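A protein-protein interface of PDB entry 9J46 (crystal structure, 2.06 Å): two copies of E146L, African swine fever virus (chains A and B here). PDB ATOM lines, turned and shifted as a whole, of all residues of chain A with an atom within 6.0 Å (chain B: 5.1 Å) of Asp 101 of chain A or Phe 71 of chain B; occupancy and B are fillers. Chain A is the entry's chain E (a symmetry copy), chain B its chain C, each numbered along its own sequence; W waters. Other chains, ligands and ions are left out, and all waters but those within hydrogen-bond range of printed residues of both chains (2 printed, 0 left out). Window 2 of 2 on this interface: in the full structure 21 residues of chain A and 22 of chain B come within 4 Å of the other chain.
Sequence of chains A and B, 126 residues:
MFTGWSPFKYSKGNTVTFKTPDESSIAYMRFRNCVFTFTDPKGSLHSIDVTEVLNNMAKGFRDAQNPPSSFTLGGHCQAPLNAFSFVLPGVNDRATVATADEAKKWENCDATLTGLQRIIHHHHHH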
ATOM      1  N   THR A  99       8.491 -16.793  -6.457  1.00  0.00           N
ATOM      2  CA  THR A  99       8.414 -17.021  -5.018  1.00  0.00           C
ATOM      3  C   THR A  99       9.490 -16.211  -4.310  1.00  0.00           C
ATOM      4  O   THR A  99      10.419 -15.696  -4.935  1.00  0.00           O
ATOM      5  CB  THR A  99       8.560 -18.514  -4.669  1.00  0.00           C
ATOM      6  OG1 THR A  99       9.826 -19.005  -5.121  1.00  0.00           O
ATOM      7  CG2 THR A  99       7.461 -19.336  -5.341  1.00  0.00           C
ATOM      8  N   ALA A 100       9.341 -16.073  -2.991  1.00  0.00           N
ATOM      9  CA  ALA A 100      10.365 -15.378  -2.217  1.00  0.00           C
ATOM     10  C   ALA A 100      11.638 -16.206  -2.123  1.00  0.00           C
ATOM     11  O   ALA A 100      12.736 -15.650  -2.015  1.00  0.00           O
ATOM     12  CB  ALA A 100       9.843 -15.042  -0.820  1.00  0.00           C
ATOM     13  N   ASP A 101      11.504 -17.532  -2.146  1.00  0.00           N
ATOM     14  CA  ASP A 101      12.670 -18.399  -2.197  1.00  0.00           C
ATOM     15  C   ASP A 101      13.506 -18.091  -3.432  1.00  0.00           C
ATOM     16  O   ASP A 101      14.717 -17.852  -3.342  1.00  0.00           O
ATOM     17  CB  ASP A 101      12.214 -19.858  -2.192  1.00  0.00           C
ATOM     18  CG  ASP A 101      11.097 -20.123  -1.163  1.00  0.00           C
ATOM     19  OD1 ASP A 101       9.915 -19.821  -1.480  1.00  0.00           O
ATOM     20  OD2 ASP A 101      11.396 -20.660  -0.062  1.00  0.00           O
ATOM     21  N   GLU A 102      12.863 -18.054  -4.596  1.00  0.00           N
ATOM     22  CA  GLU A 102      13.589 -17.771  -5.828  1.00  0.00           C
ATOM     23  C   GLU A 102      14.150 -16.356  -5.821  1.00  0.00           C
ATOM     24  O   GLU A 102      15.322 -16.139  -6.134  1.00  0.00           O
ATOM     25  CB  GLU A 102      12.668 -18.003  -7.027  1.00  0.00           C
ATOM     26  CG  GLU A 102      13.390 -18.050  -8.347  1.00  0.00           C
ATOM     27  CD  GLU A 102      14.339 -19.227  -8.439  1.00  0.00           C
ATOM     28  OE1 GLU A 102      14.170 -20.202  -7.665  1.00  0.00           O
ATOM     29  OE2 GLU A 102      15.257 -19.165  -9.287  1.00  0.00           O
ATOM     30  N   ALA A 103      13.329 -15.378  -5.434  1.00  0.00           N
ATOM     31  CA  ALA A 103      13.774 -13.990  -5.456  1.00  0.00           C
ATOM     32  C   ALA A 103      14.968 -13.764  -4.539  1.00  0.00           C
ATOM     33  O   ALA A 103      15.787 -12.871  -4.794  1.00  0.00           O
ATOM     34  CB  ALA A 103      12.624 -13.061  -5.064  1.00  0.00           C
ATOM     35  N   LYS A 104      15.092 -14.562  -3.474  1.00  0.00           N
ATOM     36  CA  LYS A 104      16.233 -14.406  -2.580  1.00  0.00           C
ATOM     37  C   LYS A 104      17.544 -14.769  -3.266  1.00  0.00           C
ATOM     38  O   LYS A 104      18.579 -14.183  -2.947  1.00  0.00           O
ATOM     39  CB  LYS A 104      16.053 -15.252  -1.323  1.00  0.00           C
ATOM     40  CG  LYS A 104      16.961 -14.812  -0.194  1.00  0.00           C
ATOM     41  CD  LYS A 104      17.436 -15.989   0.653  1.00  0.00           C
ATOM     42  CE  LYS A 104      18.178 -15.501   1.900  1.00  0.00           C
ATOM     43  NZ  LYS A 104      17.384 -14.479   2.649  1.00  0.00           N
ATOM     44  N   LYS A 105      17.521 -15.726  -4.200  1.00  0.00           N
ATOM     45  CA  LYS A 105      18.710 -16.077  -4.966  1.00  0.00           C
ATOM     46  C   LYS A 105      19.238 -14.918  -5.789  1.00  0.00           C
ATOM     47  O   LYS A 105      20.328 -15.034  -6.362  1.00  0.00           O
ATOM     48  CB  LYS A 105      18.417 -17.217  -5.932  1.00  0.00           C
ATOM     49  CG  LYS A 105      18.125 -18.557  -5.336  1.00  0.00           C
ATOM     50  CD  LYS A 105      17.427 -19.421  -6.376  1.00  0.00           C
ATOM     51  CE  LYS A 105      17.469 -20.877  -6.012  1.00  0.00           C
ATOM     52  NZ  LYS A 105      17.406 -21.043  -4.542  1.00  0.00           N
ATOM     53  N   VAL B  16       3.175 -15.699   3.835  1.00  0.00           N
ATOM     54  CA  VAL B  16       2.367 -16.777   3.287  1.00  0.00           C
ATOM     55  C   VAL B  16       3.303 -17.876   2.829  1.00  0.00           C
ATOM     56  O   VAL B  16       3.943 -17.764   1.774  1.00  0.00           O
ATOM     57  CB  VAL B  16       1.477 -16.296   2.140  1.00  0.00           C
ATOM     58  CG1 VAL B  16       0.581 -17.424   1.678  1.00  0.00           C
ATOM     59  CG2 VAL B  16       0.659 -15.093   2.600  1.00  0.00           C
ATOM     60  N   THR B  17       3.365 -18.946   3.612  1.00  0.00           N
ATOM     61  CA  THR B  17       4.205 -20.102   3.331  1.00  0.00           C
ATOM     62  C   THR B  17       3.310 -21.319   3.219  1.00  0.00           C
ATOM     63  O   THR B  17       2.576 -21.644   4.158  1.00  0.00           O
ATOM     64  CB  THR B  17       5.249 -20.306   4.437  1.00  0.00           C
ATOM     65  OG1 THR B  17       6.097 -19.160   4.493  1.00  0.00           O
ATOM     66  CG2 THR B  17       6.090 -21.534   4.175  1.00  0.00           C
ATOM     67  N   PHE B  18       3.363 -21.987   2.078  1.00  0.00           N
ATOM     68  CA  PHE B  18       2.649 -23.236   1.888  1.00  0.00           C
ATOM     69  C   PHE B  18       3.628 -24.367   2.156  1.00  0.00           C
ATOM     70  O   PHE B  18       4.674 -24.437   1.507  1.00  0.00           O
ATOM     71  CB  PHE B  18       2.066 -23.303   0.474  1.00  0.00           C
ATOM     72  CG  PHE B  18       1.015 -22.258   0.215  1.00  0.00           C
ATOM     73  CD1 PHE B  18      -0.302 -22.472   0.605  1.00  0.00           C
ATOM     74  CD2 PHE B  18       1.346 -21.054  -0.387  1.00  0.00           C
ATOM     75  CE1 PHE B  18      -1.273 -21.512   0.385  1.00  0.00           C
ATOM     76  CE2 PHE B  18       0.383 -20.085  -0.617  1.00  0.00           C
ATOM     77  CZ  PHE B  18      -0.934 -20.314  -0.228  1.00  0.00           C
ATOM     78  N   ILE B  26       7.016 -30.064  -1.909  1.00  0.00           N
ATOM     79  CA  ILE B  26       5.903 -29.085  -2.095  1.00  0.00           C
ATOM     80  C   ILE B  26       5.364 -29.198  -3.534  1.00  0.00           C
ATOM     81  O   ILE B  26       4.236 -28.717  -3.781  1.00  0.00           O
ATOM     82  CB  ILE B  26       6.369 -27.658  -1.743  1.00  0.00           C
ATOM     83  CG1 ILE B  26       5.198 -26.770  -1.319  1.00  0.00           C
ATOM     84  CG2 ILE B  26       7.179 -27.035  -2.880  1.00  0.00           C
ATOM     85  CD1 ILE B  26       4.271 -27.417  -0.307  1.00  0.00           C
ATOM     86  N   PHE B  31      -4.067 -26.590  -5.678  1.00  0.00           N
ATOM     87  CA  PHE B  31      -4.901 -25.505  -5.193  1.00  0.00           C
ATOM     88  C   PHE B  31      -6.181 -25.452  -6.009  1.00  0.00           C
ATOM     89  O   PHE B  31      -6.240 -25.934  -7.144  1.00  0.00           O
ATOM     90  CB  PHE B  31      -4.182 -24.143  -5.276  1.00  0.00           C
ATOM     91  CG  PHE B  31      -2.907 -24.088  -4.497  1.00  0.00           C
ATOM     92  CD1 PHE B  31      -1.719 -24.533  -5.053  1.00  0.00           C
ATOM     93  CD2 PHE B  31      -2.892 -23.603  -3.193  1.00  0.00           C
ATOM     94  CE1 PHE B  31      -0.529 -24.495  -4.324  1.00  0.00           C
ATOM     95  CE2 PHE B  31      -1.702 -23.557  -2.464  1.00  0.00           C
ATOM     96  CZ  PHE B  31      -0.516 -24.011  -3.044  1.00  0.00           C
ATOM     97  N   LEU B  54      -0.831 -20.139  -8.154  1.00  0.00           N
ATOM     98  CA  LEU B  54      -0.315 -20.934  -7.047  1.00  0.00           C
ATOM     99  C   LEU B  54       0.033 -22.342  -7.505  1.00  0.00           C
ATOM    100  O   LEU B  54       1.033 -22.913  -7.057  1.00  0.00           O
ATOM    101  CB  LEU B  54      -1.341 -20.971  -5.909  1.00  0.00           C
ATOM    102  CG  LEU B  54      -1.540 -19.615  -5.233  1.00  0.00           C
ATOM    103  CD1 LEU B  54      -2.698 -19.650  -4.231  1.00  0.00           C
ATOM    104  CD2 LEU B  54      -0.239 -19.168  -4.570  1.00  0.00           C
ATOM    105  N   MET B  57       3.256 -22.192  -9.142  1.00  0.00           N
ATOM    106  CA  MET B  57       4.390 -22.079  -8.221  1.00  0.00           C
ATOM    107  C   MET B  57       4.799 -23.444  -7.699  1.00  0.00           C
ATOM    108  O   MET B  57       5.992 -23.758  -7.648  1.00  0.00           O
ATOM    109  CB  MET B  57       4.104 -21.148  -7.047  1.00  0.00           C
ATOM    110  CG  MET B  57       3.928 -19.717  -7.425  1.00  0.00           C
ATOM    111  SD  MET B  57       3.296 -18.755  -6.052  1.00  0.00           S
ATOM    112  CE  MET B  57       3.274 -17.094  -6.733  1.00  0.00           C
ATOM    113  N   ALA B  58       3.821 -24.275  -7.321  1.00  0.00           N
ATOM    114  CA  ALA B  58       4.136 -25.624  -6.866  1.00  0.00           C
ATOM    115  C   ALA B  58       4.745 -26.455  -7.986  1.00  0.00           C
ATOM    116  O   ALA B  58       5.736 -27.158  -7.771  1.00  0.00           O
ATOM    117  CB  ALA B  58       2.886 -26.312  -6.328  1.00  0.00           C
ATOM    118  N   PHE B  61       8.630 -26.796  -8.870  1.00  0.00           N
ATOM    119  CA  PHE B  61       9.581 -27.658  -8.184  1.00  0.00           C
ATOM    120  C   PHE B  61       9.523 -29.093  -8.694  1.00  0.00           C
ATOM    121  O   PHE B  61      10.178 -29.972  -8.133  1.00  0.00           O
ATOM    122  CB  PHE B  61       9.342 -27.613  -6.669  1.00  0.00           C
ATOM    123  CG  PHE B  61       9.473 -26.245  -6.077  1.00  0.00           C
ATOM    124  CD1 PHE B  61      10.714 -25.758  -5.700  1.00  0.00           C
ATOM    125  CD2 PHE B  61       8.352 -25.439  -5.893  1.00  0.00           C
ATOM    126  CE1 PHE B  61      10.841 -24.497  -5.149  1.00  0.00           C
ATOM    127  CE2 PHE B  61       8.474 -24.167  -5.351  1.00  0.00           C
ATOM    128  CZ  PHE B  61       9.713 -23.695  -4.973  1.00  0.00           C
ATOM    129  N   SER B  69      10.047 -28.589   0.957  1.00  0.00           N
ATOM    130  CA  SER B  69       8.732 -28.948   1.469  1.00  0.00           C
ATOM    131  C   SER B  69       7.838 -27.726   1.630  1.00  0.00           C
ATOM    132  O   SER B  69       6.746 -27.833   2.195  1.00  0.00           O
ATOM    133  CB  SER B  69       8.872 -29.679   2.807  1.00  0.00           C
ATOM    134  OG  SER B  69       9.499 -28.835   3.756  1.00  0.00           O
ATOM    135  N   SER B  70       8.285 -26.568   1.153  1.00  0.00           N
ATOM    136  CA  SER B  70       7.498 -25.357   1.263  1.00  0.00           C
ATOM    137  C   SER B  70       7.900 -24.396   0.157  1.00  0.00           C
ATOM    138  O   SER B  70       8.949 -24.552  -0.475  1.00  0.00           O
ATOM    139  CB  SER B  70       7.693 -24.700   2.626  1.00  0.00           C
ATOM    140  OG  SER B  70       8.940 -24.042   2.664  1.00  0.00           O
ATOM    141  N   PHE B  71       7.038 -23.410  -0.086  1.00  0.00           N
ATOM    142  CA  PHE B  71       7.428 -22.206  -0.805  1.00  0.00           C
ATOM    143  C   PHE B  71       6.682 -21.031  -0.194  1.00  0.00           C
ATOM    144  O   PHE B  71       5.618 -21.195   0.411  1.00  0.00           O
ATOM    145  CB  PHE B  71       7.181 -22.311  -2.328  1.00  0.00           C
ATOM    146  CG  PHE B  71       5.727 -22.362  -2.732  1.00  0.00           C
ATOM    147  CD1 PHE B  71       4.960 -21.210  -2.802  1.00  0.00           C
ATOM    148  CD2 PHE B  71       5.143 -23.564  -3.088  1.00  0.00           C
ATOM    149  CE1 PHE B  71       3.636 -21.261  -3.196  1.00  0.00           C
ATOM    150  CE2 PHE B  71       3.819 -23.629  -3.481  1.00  0.00           C
ATOM    151  CZ  PHE B  71       3.062 -22.469  -3.546  1.00  0.00           C
ATOM    152  N   THR B  72       7.250 -19.839  -0.370  1.00  0.00           N
ATOM    153  CA  THR B  72       6.786 -18.615   0.270  1.00  0.00           C
ATOM    154  C   THR B  72       6.525 -17.544  -0.784  1.00  0.00           C
ATOM    155  O   THR B  72       7.346 -17.353  -1.684  1.00  0.00           O
ATOM    156  CB  THR B  72       7.841 -18.151   1.282  1.00  0.00           C
ATOM    157  OG1 THR B  72       7.898 -19.092   2.362  1.00  0.00           O
ATOM    158  CG2 THR B  72       7.555 -16.755   1.813  1.00  0.00           C
ATOM    159  N   LEU B  73       5.376 -16.868  -0.692  1.00  0.00           N
ATOM    160  CA  LEU B  73       5.096 -15.728  -1.555  1.00  0.00           C
ATOM    161  C   LEU B  73       5.991 -14.553  -1.189  1.00  0.00           C
ATOM    162  O   LEU B  73       6.349 -14.363  -0.025  1.00  0.00           O
ATOM    163  CB  LEU B  73       3.634 -15.285  -1.430  1.00  0.00           C
ATOM    164  CG  LEU B  73       2.485 -16.285  -1.444  1.00  0.00           C
ATOM    165  CD1 LEU B  73       1.172 -15.519  -1.459  1.00  0.00           C
ATOM    166  CD2 LEU B  73       2.592 -17.178  -2.677  1.00  0.00           C
HETATM  167  O   HOH W   1      11.348 -23.232  -1.231  1.00  0.00           O
HETATM  168  O   HOH W   2       9.423 -21.433   1.608  1.00  0.00           O
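Water W2 lies within hydrogen-bond range of OD2 of Asp 101 of chain A (2.7 Å), OG of Ser 70 of chain B (2.9 Å) and OG1 of Thr 72 of chain B (2.9 Å).
Water W1 bridges OD2 of Asp 101 of chain A (2.8 Å) and O of Ser 70 of chain B (2.8 Å).
Among the printed residues, pairs that only touch across the chains: Thr 99 of chain A with Thr 72 of chain B (3.4 Å), Ala 100 of chain A with Leu 73 of chain B (3.6 Å) and Asp 101 of chain A with Phe 71 of chain B (3.5 Å).
Of the 7 printed residues of chain A, 3 touch a printed residue of chain B.
Printed residues of chain A that touch a printed residue of chain B: Thr 99, Ala 100 and Asp 101.
Hydrophobic or aromatic side chains of chain B within 4 Å of the printed part of chain A: Phe 71.
Among the printed residues, 5 pairs touch across the chains.
Among the printed residues, no Asp or Glu carboxylate lies within 4 Å of a Lys or Arg side-chain nitrogen of the other chain.
No position is printed for both chains.
The backbone NH (N) of Phe 18 of chain B sits at hydrogen-bond distance from the backbone carbonyl oxygen (O) of Phe 71 of chain B (2.9 Å).
The backbone carbonyl oxygen (O) of Val 16 of chain B sits at hydrogen-bond distance from the backbone NH (N) of Leu 73 of chain B, at 3.0 Å.
OG1 of Thr 17 of chain B sits at hydrogen-bond distance from OG1 of Thr 72 of chain B (2.8 Å).
The side-chain hydroxyl (OG1) of Thr 99 of chain A lies within hydrogen-bond range of the backbone NH (N) of Glu 102 of chain A (3.2 Å).
Phe 71 of chain B touches one residue of chain A.
Of the printed residues of chain B, Ala 100 of chain A touches Thr 72 and Leu 73.
Printed residues of chain A within 4 Å of Thr 72 of chain B: Thr 99 (3.4 Å), Ala 100 (2.7 Å) and Asp 101 (2.9 Å).
Printed residues of chain A within 4 Å of Leu 73 of chain B: Ala 100.
Of the printed residues of chain B, Thr 99 of chain A touches Thr 72.
Ser 69 of chain B touches none of the printed residues of chain A.
The nearest residue of chain B that does not touch Asp 101 of chain A is Ser 70 of chain B (4.6 Å).
The nearest residue of chain A that does not touch Phe 71 of chain B is Thr 99 of chain A (4.03 Å).
N of Thr 72 of chain B lies within hydrogen-bond range of OD1 of Asp 101 of chain A (2.9 Å).
The backbone carbonyl oxygen (O) of Thr 72 of chain B sits at hydrogen-bond distance from the backbone NH (N) of Ala 100 of chain A (2.7 Å).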
